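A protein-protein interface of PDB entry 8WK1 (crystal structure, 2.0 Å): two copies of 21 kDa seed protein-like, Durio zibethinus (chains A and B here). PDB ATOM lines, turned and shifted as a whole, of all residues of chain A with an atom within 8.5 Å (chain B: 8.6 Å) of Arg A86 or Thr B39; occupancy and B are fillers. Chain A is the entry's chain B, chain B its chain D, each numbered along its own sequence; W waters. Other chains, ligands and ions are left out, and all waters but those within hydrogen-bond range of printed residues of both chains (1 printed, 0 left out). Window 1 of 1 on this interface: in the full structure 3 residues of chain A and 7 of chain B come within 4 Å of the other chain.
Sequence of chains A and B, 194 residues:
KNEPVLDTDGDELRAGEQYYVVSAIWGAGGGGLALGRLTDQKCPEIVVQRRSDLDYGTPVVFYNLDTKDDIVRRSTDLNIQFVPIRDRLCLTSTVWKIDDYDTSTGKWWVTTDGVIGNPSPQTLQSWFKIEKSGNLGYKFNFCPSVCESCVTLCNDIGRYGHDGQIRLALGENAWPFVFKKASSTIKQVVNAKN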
ATOM      1  N   ALA A  34      -7.805  16.210 -12.826  1.00  0.00           N
ATOM      2  CA  ALA A  34      -7.375  17.547 -12.457  1.00  0.00           C
ATOM      3  C   ALA A  34      -8.095  17.968 -11.193  1.00  0.00           C
ATOM      4  O   ALA A  34      -9.135  17.408 -10.837  1.00  0.00           O
ATOM      5  CB  ALA A  34      -7.668  18.562 -13.575  1.00  0.00           C
ATOM      6  N   LEU A  35      -7.544  18.978 -10.528  1.00  0.00           N
ATOM      7  CA  LEU A  35      -8.283  19.656  -9.474  1.00  0.00           C
ATOM      8  C   LEU A  35      -9.412  20.466 -10.087  1.00  0.00           C
ATOM      9  O   LEU A  35      -9.185  21.238 -11.021  1.00  0.00           O
ATOM     10  CB  LEU A  35      -7.371  20.592  -8.704  1.00  0.00           C
ATOM     11  CG  LEU A  35      -6.557  20.012  -7.576  1.00  0.00           C
ATOM     12  CD1 LEU A  35      -5.474  21.017  -7.226  1.00  0.00           C
ATOM     13  CD2 LEU A  35      -7.475  19.719  -6.398  1.00  0.00           C
ATOM     14  N   GLY A  36     -10.619  20.304  -9.558  1.00  0.00           N
ATOM     15  CA  GLY A  36     -11.752  21.071 -10.026  1.00  0.00           C
ATOM     16  C   GLY A  36     -12.574  21.626  -8.880  1.00  0.00           C
ATOM     17  O   GLY A  36     -12.190  21.509  -7.714  1.00  0.00           O
ATOM     18  N   ARG A  37     -13.712  22.234  -9.192  1.00  0.00           N
ATOM     19  CA  ARG A  37     -14.610  22.651  -8.128  1.00  0.00           C
ATOM     20  C   ARG A  37     -16.040  22.513  -8.617  1.00  0.00           C
ATOM     21  O   ARG A  37     -16.299  22.389  -9.819  1.00  0.00           O
ATOM     22  CB  ARG A  37     -14.333  24.087  -7.676  1.00  0.00           C
ATOM     23  CG  ARG A  37     -14.263  25.074  -8.826  1.00  0.00           C
ATOM     24  CD  ARG A  37     -14.635  26.484  -8.375  1.00  0.00           C
ATOM     25  NE  ARG A  37     -16.005  26.566  -7.877  1.00  0.00           N
ATOM     26  CZ  ARG A  37     -16.507  27.621  -7.247  1.00  0.00           C
ATOM     27  NH1 ARG A  37     -15.773  28.698  -7.005  1.00  0.00           N
ATOM     28  NH2 ARG A  37     -17.776  27.592  -6.842  1.00  0.00           N
ATOM     29  N   GLU A  45     -11.628  21.459  -3.039  1.00  0.00           N
ATOM     30  CA  GLU A  45     -11.697  21.143  -4.451  1.00  0.00           C
ATOM     31  C   GLU A  45     -12.049  19.667  -4.646  1.00  0.00           C
ATOM     32  O   GLU A  45     -11.861  18.837  -3.760  1.00  0.00           O
ATOM     33  CB  GLU A  45     -10.370  21.497  -5.116  1.00  0.00           C
ATOM     34  CG  GLU A  45     -10.084  22.982  -5.046  1.00  0.00           C
ATOM     35  CD  GLU A  45      -8.613  23.308  -4.897  1.00  0.00           C
ATOM     36  OE1 GLU A  45      -8.000  22.944  -3.859  1.00  0.00           O
ATOM     37  OE2 GLU A  45      -8.075  23.947  -5.822  1.00  0.00           O
ATOM     38  N   ARG A  50     -10.542  15.835 -17.228  1.00  0.00           N
ATOM     39  CA  ARG A  50     -10.583  16.673 -18.420  1.00  0.00           C
ATOM     40  C   ARG A  50     -11.275  15.920 -19.550  1.00  0.00           C
ATOM     41  O   ARG A  50     -11.058  14.715 -19.742  1.00  0.00           O
ATOM     42  CB  ARG A  50      -9.172  17.070 -18.846  1.00  0.00           C
ATOM     43  CG  ARG A  50      -8.447  17.945 -17.865  1.00  0.00           C
ATOM     44  CD  ARG A  50      -9.150  19.271 -17.679  1.00  0.00           C
ATOM     45  NE  ARG A  50      -8.368  20.189 -16.855  1.00  0.00           N
ATOM     46  CZ  ARG A  50      -8.847  20.865 -15.820  1.00  0.00           C
ATOM     47  NH1 ARG A  50     -10.099  20.728 -15.420  1.00  0.00           N
ATOM     48  NH2 ARG A  50      -8.047  21.706 -15.171  1.00  0.00           N
ATOM     49  N   ASP A  55      -5.467  17.020 -22.916  1.00  0.00           N
ATOM     50  CA  ASP A  55      -5.282  17.711 -21.645  1.00  0.00           C
ATOM     51  C   ASP A  55      -5.061  16.674 -20.555  1.00  0.00           C
ATOM     52  O   ASP A  55      -5.994  15.960 -20.167  1.00  0.00           O
ATOM     53  CB  ASP A  55      -6.493  18.585 -21.337  1.00  0.00           C
ATOM     54  CG  ASP A  55      -6.242  19.564 -20.207  1.00  0.00           C
ATOM     55  OD1 ASP A  55      -5.281  19.369 -19.428  1.00  0.00           O
ATOM     56  OD2 ASP A  55      -7.020  20.533 -20.093  1.00  0.00           O
ATOM     57  N   THR A  58      -3.880  17.740 -13.860  1.00  0.00           N
ATOM     58  CA  THR A  58      -2.980  18.156 -12.798  1.00  0.00           C
ATOM     59  C   THR A  58      -2.111  16.980 -12.385  1.00  0.00           C
ATOM     60  O   THR A  58      -2.642  15.883 -12.170  1.00  0.00           O
ATOM     61  CB  THR A  58      -3.780  18.661 -11.583  1.00  0.00           C
ATOM     62  OG1 THR A  58      -4.807  19.564 -12.011  1.00  0.00           O
ATOM     63  CG2 THR A  58      -2.877  19.363 -10.573  1.00  0.00           C
ATOM     64  N   PRO A  59      -0.794  17.147 -12.261  1.00  0.00           N
ATOM     65  CA  PRO A  59       0.039  16.028 -11.803  1.00  0.00           C
ATOM     66  C   PRO A  59      -0.294  15.627 -10.369  1.00  0.00           C
ATOM     67  O   PRO A  59      -0.788  16.428  -9.574  1.00  0.00           O
ATOM     68  CB  PRO A  59       1.475  16.563 -11.914  1.00  0.00           C
ATOM     69  CG  PRO A  59       1.390  17.950 -12.421  1.00  0.00           C
ATOM     70  CD  PRO A  59      -0.032  18.377 -12.531  1.00  0.00           C
ATOM     71  N   VAL A  83      -0.601  17.929  -7.271  1.00  0.00           N
ATOM     72  CA  VAL A  83       0.432  18.939  -7.076  1.00  0.00           C
ATOM     73  C   VAL A  83       0.162  20.067  -8.064  1.00  0.00           C
ATOM     74  O   VAL A  83       0.722  20.070  -9.170  1.00  0.00           O
ATOM     75  CB  VAL A  83       1.829  18.332  -7.257  1.00  0.00           C
ATOM     76  CG1 VAL A  83       2.905  19.410  -7.196  1.00  0.00           C
ATOM     77  CG2 VAL A  83       2.067  17.270  -6.194  1.00  0.00           C
ATOM     78  N   PRO A  84      -0.700  21.021  -7.736  1.00  0.00           N
ATOM     79  CA  PRO A  84      -1.062  22.046  -8.718  1.00  0.00           C
ATOM     80  C   PRO A  84       0.095  22.993  -8.977  1.00  0.00           C
ATOM     81  O   PRO A  84       0.987  23.184  -8.146  1.00  0.00           O
ATOM     82  CB  PRO A  84      -2.231  22.774  -8.055  1.00  0.00           C
ATOM     83  CG  PRO A  84      -1.928  22.662  -6.584  1.00  0.00           C
ATOM     84  CD  PRO A  84      -1.217  21.332  -6.393  1.00  0.00           C
ATOM     85  N   ILE A  85       0.086  23.579 -10.167  1.00  0.00           N
ATOM     86  CA  ILE A  85       1.042  24.642 -10.448  1.00  0.00           C
ATOM     87  C   ILE A  85       0.463  26.010 -10.102  1.00  0.00           C
ATOM     88  O   ILE A  85       1.189  26.876  -9.606  1.00  0.00           O
ATOM     89  CB  ILE A  85       1.500  24.568 -11.912  1.00  0.00           C
ATOM     90  CG1 ILE A  85       2.662  25.529 -12.167  1.00  0.00           C
ATOM     91  CG2 ILE A  85       0.331  24.843 -12.862  1.00  0.00           C
ATOM     92  CD1 ILE A  85       3.609  25.056 -13.243  1.00  0.00           C
ATOM     93  N   ARG A  86      -0.847  26.193 -10.281  1.00  0.00           N
ATOM     94  CA  ARG A  86      -1.527  27.460 -10.047  1.00  0.00           C
ATOM     95  C   ARG A  86      -1.452  27.913  -8.591  1.00  0.00           C
ATOM     96  O   ARG A  86      -0.925  27.202  -7.724  1.00  0.00           O
ATOM     97  CB  ARG A  86      -2.997  27.338 -10.459  1.00  0.00           C
ATOM     98  CG  ARG A  86      -3.240  27.196 -11.953  1.00  0.00           C
ATOM     99  CD  ARG A  86      -3.262  28.549 -12.647  1.00  0.00           C
ATOM    100  NE  ARG A  86      -3.443  28.409 -14.087  1.00  0.00           N
ATOM    101  CZ  ARG A  86      -4.399  29.004 -14.786  1.00  0.00           C
ATOM    102  NH1 ARG A  86      -5.282  29.800 -14.207  1.00  0.00           N
ATOM    103  NH2 ARG A  86      -4.472  28.795 -16.098  1.00  0.00           N
ATOM    104  N   ASP A  87      -1.996  29.100  -8.323  1.00  0.00           N
ATOM    105  CA  ASP A  87      -2.162  29.590  -6.958  1.00  0.00           C
ATOM    106  C   ASP A  87      -3.094  28.667  -6.172  1.00  0.00           C
ATOM    107  O   ASP A  87      -3.967  28.002  -6.740  1.00  0.00           O
ATOM    108  CB  ASP A  87      -2.722  31.018  -6.988  1.00  0.00           C
ATOM    109  CG  ASP A  87      -2.541  31.755  -5.674  1.00  0.00           C
ATOM    110  OD1 ASP A  87      -1.849  31.222  -4.775  1.00  0.00           O
ATOM    111  OD2 ASP A  87      -3.089  32.875  -5.544  1.00  0.00           O
ATOM    112  N   ARG A  88      -2.904  28.624  -4.852  1.00  0.00           N
ATOM    113  CA  ARG A  88      -3.709  27.775  -3.977  1.00  0.00           C
ATOM    114  C   ARG A  88      -4.954  28.543  -3.550  1.00  0.00           C
ATOM    115  O   ARG A  88      -4.885  29.426  -2.691  1.00  0.00           O
ATOM    116  CB  ARG A  88      -2.895  27.319  -2.770  1.00  0.00           C
ATOM    117  CG  ARG A  88      -2.010  26.113  -3.074  1.00  0.00           C
ATOM    118  CD  ARG A  88      -2.465  24.866  -2.325  1.00  0.00           C
ATOM    119  NE  ARG A  88      -3.843  24.493  -2.629  1.00  0.00           N
ATOM    120  CZ  ARG A  88      -4.643  23.865  -1.775  1.00  0.00           C
ATOM    121  NH1 ARG A  88      -4.211  23.486  -0.582  1.00  0.00           N
ATOM    122  NH2 ARG A  88      -5.911  23.626  -2.119  1.00  0.00           N
ATOM    123  N   LEU A  89      -6.093  28.200  -4.151  1.00  0.00           N
ATOM    124  CA  LEU A  89      -7.350  28.890  -3.892  1.00  0.00           C
ATOM    125  C   LEU A  89      -7.960  28.539  -2.540  1.00  0.00           C
ATOM    126  O   LEU A  89      -8.794  29.302  -2.038  1.00  0.00           O
ATOM    127  CB  LEU A  89      -8.368  28.560  -4.994  1.00  0.00           C
ATOM    128  CG  LEU A  89      -8.164  29.048  -6.434  1.00  0.00           C
ATOM    129  CD1 LEU A  89      -7.217  28.152  -7.231  1.00  0.00           C
ATOM    130  CD2 LEU A  89      -9.510  29.124  -7.135  1.00  0.00           C
ATOM    131  N   LEU B  35       0.234  37.914 -20.122  1.00  0.00           N
ATOM    132  CA  LEU B  35      -0.755  37.008 -20.695  1.00  0.00           C
ATOM    133  C   LEU B  35      -1.024  35.878 -19.715  1.00  0.00           C
ATOM    134  O   LEU B  35      -0.087  35.280 -19.180  1.00  0.00           O
ATOM    135  CB  LEU B  35      -0.253  36.431 -22.014  1.00  0.00           C
ATOM    136  CG  LEU B  35      -0.412  37.219 -23.299  1.00  0.00           C
ATOM    137  CD1 LEU B  35       0.441  36.543 -24.369  1.00  0.00           C
ATOM    138  CD2 LEU B  35      -1.862  37.281 -23.733  1.00  0.00           C
ATOM    139  N   GLY B  36      -2.300  35.575 -19.481  1.00  0.00           N
ATOM    140  CA  GLY B  36      -2.672  34.507 -18.575  1.00  0.00           C
ATOM    141  C   GLY B  36      -3.797  33.664 -19.148  1.00  0.00           C
ATOM    142  O   GLY B  36      -4.281  33.916 -20.250  1.00  0.00           O
ATOM    143  N   ARG B  37      -4.202  32.661 -18.367  1.00  0.00           N
ATOM    144  CA  ARG B  37      -5.234  31.694 -18.724  1.00  0.00           C
ATOM    145  C   ARG B  37      -6.151  31.464 -17.533  1.00  0.00           C
ATOM    146  O   ARG B  37      -5.689  31.371 -16.392  1.00  0.00           O
ATOM    147  CB  ARG B  37      -4.634  30.336 -19.133  1.00  0.00           C
ATOM    148  CG  ARG B  37      -4.190  30.251 -20.559  1.00  0.00           C
ATOM    149  CD  ARG B  37      -2.941  29.380 -20.710  1.00  0.00           C
ATOM    150  NE  ARG B  37      -2.029  29.963 -21.689  1.00  0.00           N
ATOM    151  CZ  ARG B  37      -1.040  30.803 -21.406  1.00  0.00           C
ATOM    152  NH1 ARG B  37      -0.716  31.099 -20.155  1.00  0.00           N
ATOM    153  NH2 ARG B  37      -0.355  31.357 -22.405  1.00  0.00           N
ATOM    154  N   LEU B  38      -7.444  31.348 -17.802  1.00  0.00           N
ATOM    155  CA  LEU B  38      -8.361  30.837 -16.797  1.00  0.00           C
ATOM    156  C   LEU B  38      -8.193  29.328 -16.651  1.00  0.00           C
ATOM    157  O   LEU B  38      -7.831  28.632 -17.605  1.00  0.00           O
ATOM    158  CB  LEU B  38      -9.804  31.163 -17.174  1.00  0.00           C
ATOM    159  CG  LEU B  38     -10.200  32.629 -17.037  1.00  0.00           C
ATOM    160  CD1 LEU B  38     -11.577  32.836 -17.658  1.00  0.00           C
ATOM    161  CD2 LEU B  38     -10.175  33.036 -15.557  1.00  0.00           C
ATOM    162  N   THR B  39      -8.468  28.819 -15.445  1.00  0.00           N
ATOM    163  CA  THR B  39      -8.322  27.383 -15.218  1.00  0.00           C
ATOM    164  C   THR B  39      -9.289  26.564 -16.073  1.00  0.00           C
ATOM    165  O   THR B  39      -8.981  25.419 -16.424  1.00  0.00           O
ATOM    166  CB  THR B  39      -8.513  27.040 -13.738  1.00  0.00           C
ATOM    167  OG1 THR B  39      -9.619  27.775 -13.207  1.00  0.00           O
ATOM    168  CG2 THR B  39      -7.255  27.357 -12.935  1.00  0.00           C
ATOM    169  N   ASP B  40     -10.445  27.123 -16.431  1.00  0.00           N
ATOM    170  CA  ASP B  40     -11.471  26.382 -17.163  1.00  0.00           C
ATOM    171  C   ASP B  40     -11.682  26.873 -18.595  1.00  0.00           C
ATOM    172  O   ASP B  40     -12.634  26.431 -19.251  1.00  0.00           O
ATOM    173  CB  ASP B  40     -12.799  26.417 -16.401  1.00  0.00           C
ATOM    174  CG  ASP B  40     -13.130  27.792 -15.872  1.00  0.00           C
ATOM    175  OD1 ASP B  40     -12.321  28.718 -16.085  1.00  0.00           O
ATOM    176  OD2 ASP B  40     -14.199  27.949 -15.246  1.00  0.00           O
ATOM    177  N   GLN B  41     -10.829  27.768 -19.096  1.00  0.00           N
ATOM    178  CA  GLN B  41     -10.884  28.207 -20.489  1.00  0.00           C
ATOM    179  C   GLN B  41      -9.463  28.465 -20.961  1.00  0.00           C
ATOM    180  O   GLN B  41      -8.750  29.285 -20.375  1.00  0.00           O
ATOM    181  CB  GLN B  41     -11.749  29.459 -20.659  1.00  0.00           C
ATOM    182  CG  GLN B  41     -11.233  30.437 -21.721  1.00  0.00           C
ATOM    183  CD  GLN B  41     -11.850  31.830 -21.620  1.00  0.00           C
ATOM    184  OE1 GLN B  41     -13.068  31.977 -21.450  1.00  0.00           O
ATOM    185  NE2 GLN B  41     -11.005  32.863 -21.713  1.00  0.00           N
ATOM    186  N   LYS B  42      -9.050  27.755 -22.014  1.00  0.00           N
ATOM    187  CA  LYS B  42      -7.678  27.860 -22.500  1.00  0.00           C
ATOM    188  C   LYS B  42      -7.481  29.091 -23.390  1.00  0.00           C
ATOM    189  O   LYS B  42      -6.415  29.724 -23.356  1.00  0.00           O
ATOM    190  CB  LYS B  42      -7.309  26.579 -23.252  1.00  0.00           C
ATOM    191  CG  LYS B  42      -6.610  25.536 -22.376  1.00  0.00           C
ATOM    192  CD  LYS B  42      -6.161  24.310 -23.170  1.00  0.00           C
ATOM    193  CE  LYS B  42      -5.422  23.308 -22.271  1.00  0.00           C
ATOM    194  NZ  LYS B  42      -4.839  22.139 -23.019  1.00  0.00           N
ATOM    195  N   ILE B  46      -6.125  35.778 -21.115  1.00  0.00           N
ATOM    196  CA  ILE B  46      -6.641  36.921 -20.384  1.00  0.00           C
ATOM    197  C   ILE B  46      -5.471  37.798 -19.962  1.00  0.00           C
ATOM    198  O   ILE B  46      -4.304  37.403 -20.030  1.00  0.00           O
ATOM    199  CB  ILE B  46      -7.481  36.497 -19.162  1.00  0.00           C
ATOM    200  CG1 ILE B  46      -6.660  35.638 -18.206  1.00  0.00           C
ATOM    201  CG2 ILE B  46      -8.759  35.768 -19.586  1.00  0.00           C
ATOM    202  CD1 ILE B  46      -7.376  35.401 -16.886  1.00  0.00           C
ATOM    203  N   VAL B  48      -3.631  39.332 -16.926  1.00  0.00           N
ATOM    204  CA  VAL B  48      -3.485  39.142 -15.489  1.00  0.00           C
ATOM    205  C   VAL B  48      -2.336  40.013 -15.003  1.00  0.00           C
ATOM    206  O   VAL B  48      -1.510  40.485 -15.788  1.00  0.00           O
ATOM    207  CB  VAL B  48      -3.237  37.663 -15.090  1.00  0.00           C
ATOM    208  CG1 VAL B  48      -4.429  36.783 -15.451  1.00  0.00           C
ATOM    209  CG2 VAL B  48      -1.953  37.140 -15.698  1.00  0.00           C
ATOM    210  N   ARG B  51       1.930  38.941  -9.091  1.00  0.00           N
ATOM    211  CA  ARG B  51       1.953  39.412  -7.710  1.00  0.00           C
ATOM    212  C   ARG B  51       3.301  40.011  -7.316  1.00  0.00           C
ATOM    213  O   ARG B  51       3.348  40.882  -6.436  1.00  0.00           O
ATOM    214  CB  ARG B  51       1.614  38.274  -6.747  1.00  0.00           C
ATOM    215  CG  ARG B  51       0.208  37.735  -6.867  1.00  0.00           C
ATOM    216  CD  ARG B  51      -0.007  36.521  -5.940  1.00  0.00           C
ATOM    217  NE  ARG B  51       0.467  36.802  -4.590  1.00  0.00           N
ATOM    218  CZ  ARG B  51       1.097  35.933  -3.805  1.00  0.00           C
ATOM    219  NH1 ARG B  51       1.341  34.690  -4.196  1.00  0.00           N
ATOM    220  NH2 ARG B  51       1.494  36.323  -2.596  1.00  0.00           N
ATOM    221  N   HIS B 162     -10.048  37.094  -9.568  1.00  0.00           N
ATOM    222  CA  HIS B 162     -10.838  36.120 -10.313  1.00  0.00           C
ATOM    223  C   HIS B 162     -10.025  34.841 -10.416  1.00  0.00           C
ATOM    224  O   HIS B 162      -8.863  34.890 -10.820  1.00  0.00           O
ATOM    225  CB  HIS B 162     -11.177  36.616 -11.733  1.00  0.00           C
ATOM    226  CG  HIS B 162     -12.188  35.770 -12.446  1.00  0.00           C
ATOM    227  ND1 HIS B 162     -12.152  35.550 -13.809  1.00  0.00           N
ATOM    228  CD2 HIS B 162     -13.280  35.107 -11.987  1.00  0.00           C
ATOM    229  CE1 HIS B 162     -13.173  34.784 -14.155  1.00  0.00           C
ATOM    230  NE2 HIS B 162     -13.872  34.502 -13.070  1.00  0.00           N
ATOM    231  N   ASP B 163     -10.629  33.703 -10.076  1.00  0.00           N
ATOM    232  CA  ASP B 163     -10.012  32.407 -10.365  1.00  0.00           C
ATOM    233  C   ASP B 163      -8.662  32.257  -9.648  1.00  0.00           C
ATOM    234  O   ASP B 163      -7.731  31.643 -10.178  1.00  0.00           O
ATOM    235  CB  ASP B 163      -9.851  32.244 -11.885  1.00  0.00           C
ATOM    236  CG  ASP B 163      -9.468  30.838 -12.305  1.00  0.00           C
ATOM    237  OD1 ASP B 163      -9.900  29.871 -11.638  1.00  0.00           O
ATOM    238  OD2 ASP B 163      -8.717  30.720 -13.310  1.00  0.00           O
ATOM    239  N   GLY B 164      -8.538  32.846  -8.456  1.00  0.00           N
ATOM    240  CA  GLY B 164      -7.276  32.905  -7.738  1.00  0.00           C
ATOM    241  C   GLY B 164      -6.201  33.793  -8.339  1.00  0.00           C
ATOM    242  O   GLY B 164      -5.057  33.754  -7.877  1.00  0.00           O
ATOM    243  N   GLN B 165      -6.532  34.598  -9.345  1.00  0.00           N
ATOM    244  CA  GLN B 165      -5.594  35.449 -10.055  1.00  0.00           C
ATOM    245  C   GLN B 165      -6.023  36.905  -9.921  1.00  0.00           C
ATOM    246  O   GLN B 165      -7.110  37.213  -9.422  1.00  0.00           O
ATOM    247  CB  GLN B 165      -5.512  35.056 -11.534  1.00  0.00           C
ATOM    248  CG  GLN B 165      -5.251  33.578 -11.768  1.00  0.00           C
ATOM    249  CD  GLN B 165      -4.932  33.299 -13.221  1.00  0.00           C
ATOM    250  OE1 GLN B 165      -3.868  33.662 -13.702  1.00  0.00           O
ATOM    251  NE2 GLN B 165      -5.860  32.668 -13.930  1.00  0.00           N
ATOM    252  N   ARG B 167      -6.916  40.133 -12.116  1.00  0.00           N
ATOM    253  CA  ARG B 167      -7.339  40.531 -13.449  1.00  0.00           C
ATOM    254  C   ARG B 167      -7.612  42.028 -13.469  1.00  0.00           C
ATOM    255  O   ARG B 167      -7.554  42.705 -12.439  1.00  0.00           O
ATOM    256  CB  ARG B 167      -8.594  39.750 -13.874  1.00  0.00           C
ATOM    257  CG  ARG B 167      -8.384  38.236 -14.037  1.00  0.00           C
ATOM    258  CD  ARG B 167      -9.591  37.609 -14.754  1.00  0.00           C
ATOM    259  NE  ARG B 167      -9.730  38.095 -16.122  1.00  0.00           N
ATOM    260  CZ  ARG B 167     -10.605  37.624 -17.003  1.00  0.00           C
ATOM    261  NH1 ARG B 167     -11.485  36.704 -16.671  1.00  0.00           N
ATOM    262  NH2 ARG B 167     -10.588  38.094 -18.249  1.00  0.00           N
HETATM  263  O   HOH W   1      -3.609  36.059  -6.746  1.00  0.00           O
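Printed residues of chain B within 4 Å of Arg A86: Arg B37, Leu B38, Thr B39, Asp B163 and Gln B165. Of the printed residues of chain B, Asp A87 touches Gly B164 (3.2 Å). Of the printed residues of chain A, Leu B38 touches Arg A86. Of the printed residues of chain A, Arg B37 touches Arg A86. Asp B40 touches none of the printed residues of chain A. Ala A34 touches none of the printed residues of chain B. The nearest residue of chain B that does not touch Arg A86 is Gly B36 (5.8 Å).
Of the 16 printed residues of chain B, 7 touch a printed residue of chain A. Among the printed residues, 7 pairs touch across the chains.
Positions printed for both chains: 35, 36 and 37. Of the 7 pairs that touch across the chains among the printed residues, none has its exchanged pair printed and touching as well.
Water W1 lies within hydrogen-bond range of O of Gly B164 and OD2 of Asp A87.
Among the printed residues, pairs that only touch across the chains: Arg A86 with Thr B39 (3.4 Å) and Arg A86 with Leu B38 (3.7 Å).
NZ of Lys B42 lies within salt-bridge range of OD2 of Asp A55 (3.99 Å). NH1 of Arg A86 lies within hydrogen-bond range of O of Arg B37 (2.7 Å). The side-chain carboxylate (OD2) of Asp B163 lies within salt-bridge range of the guanidinium group (NH1) of Arg A86, at 3.7 Å. NE2 of Gln B165 lies close to NH1 of Arg A86 (2.9 Å). The side-chain carboxylate (OD2) of Asp A87 lies close to the backbone carbonyl oxygen (O) of Gly B164 (3.2 Å).
The side-chain carboxylate (OD2) of Asp A55 is in salt-bridge range of the guanidinium group (NE) of Arg A50 (3.5 Å). The backbone carbonyl oxygen (O) of Arg B37 is in hydrogen-bond range of the side-chain amide nitrogen (NE2) of Gln B165 (2.8 Å). OG1 of Thr B39 is in hydrogen-bond range of OD1 of Asp B163 (2.6 Å).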
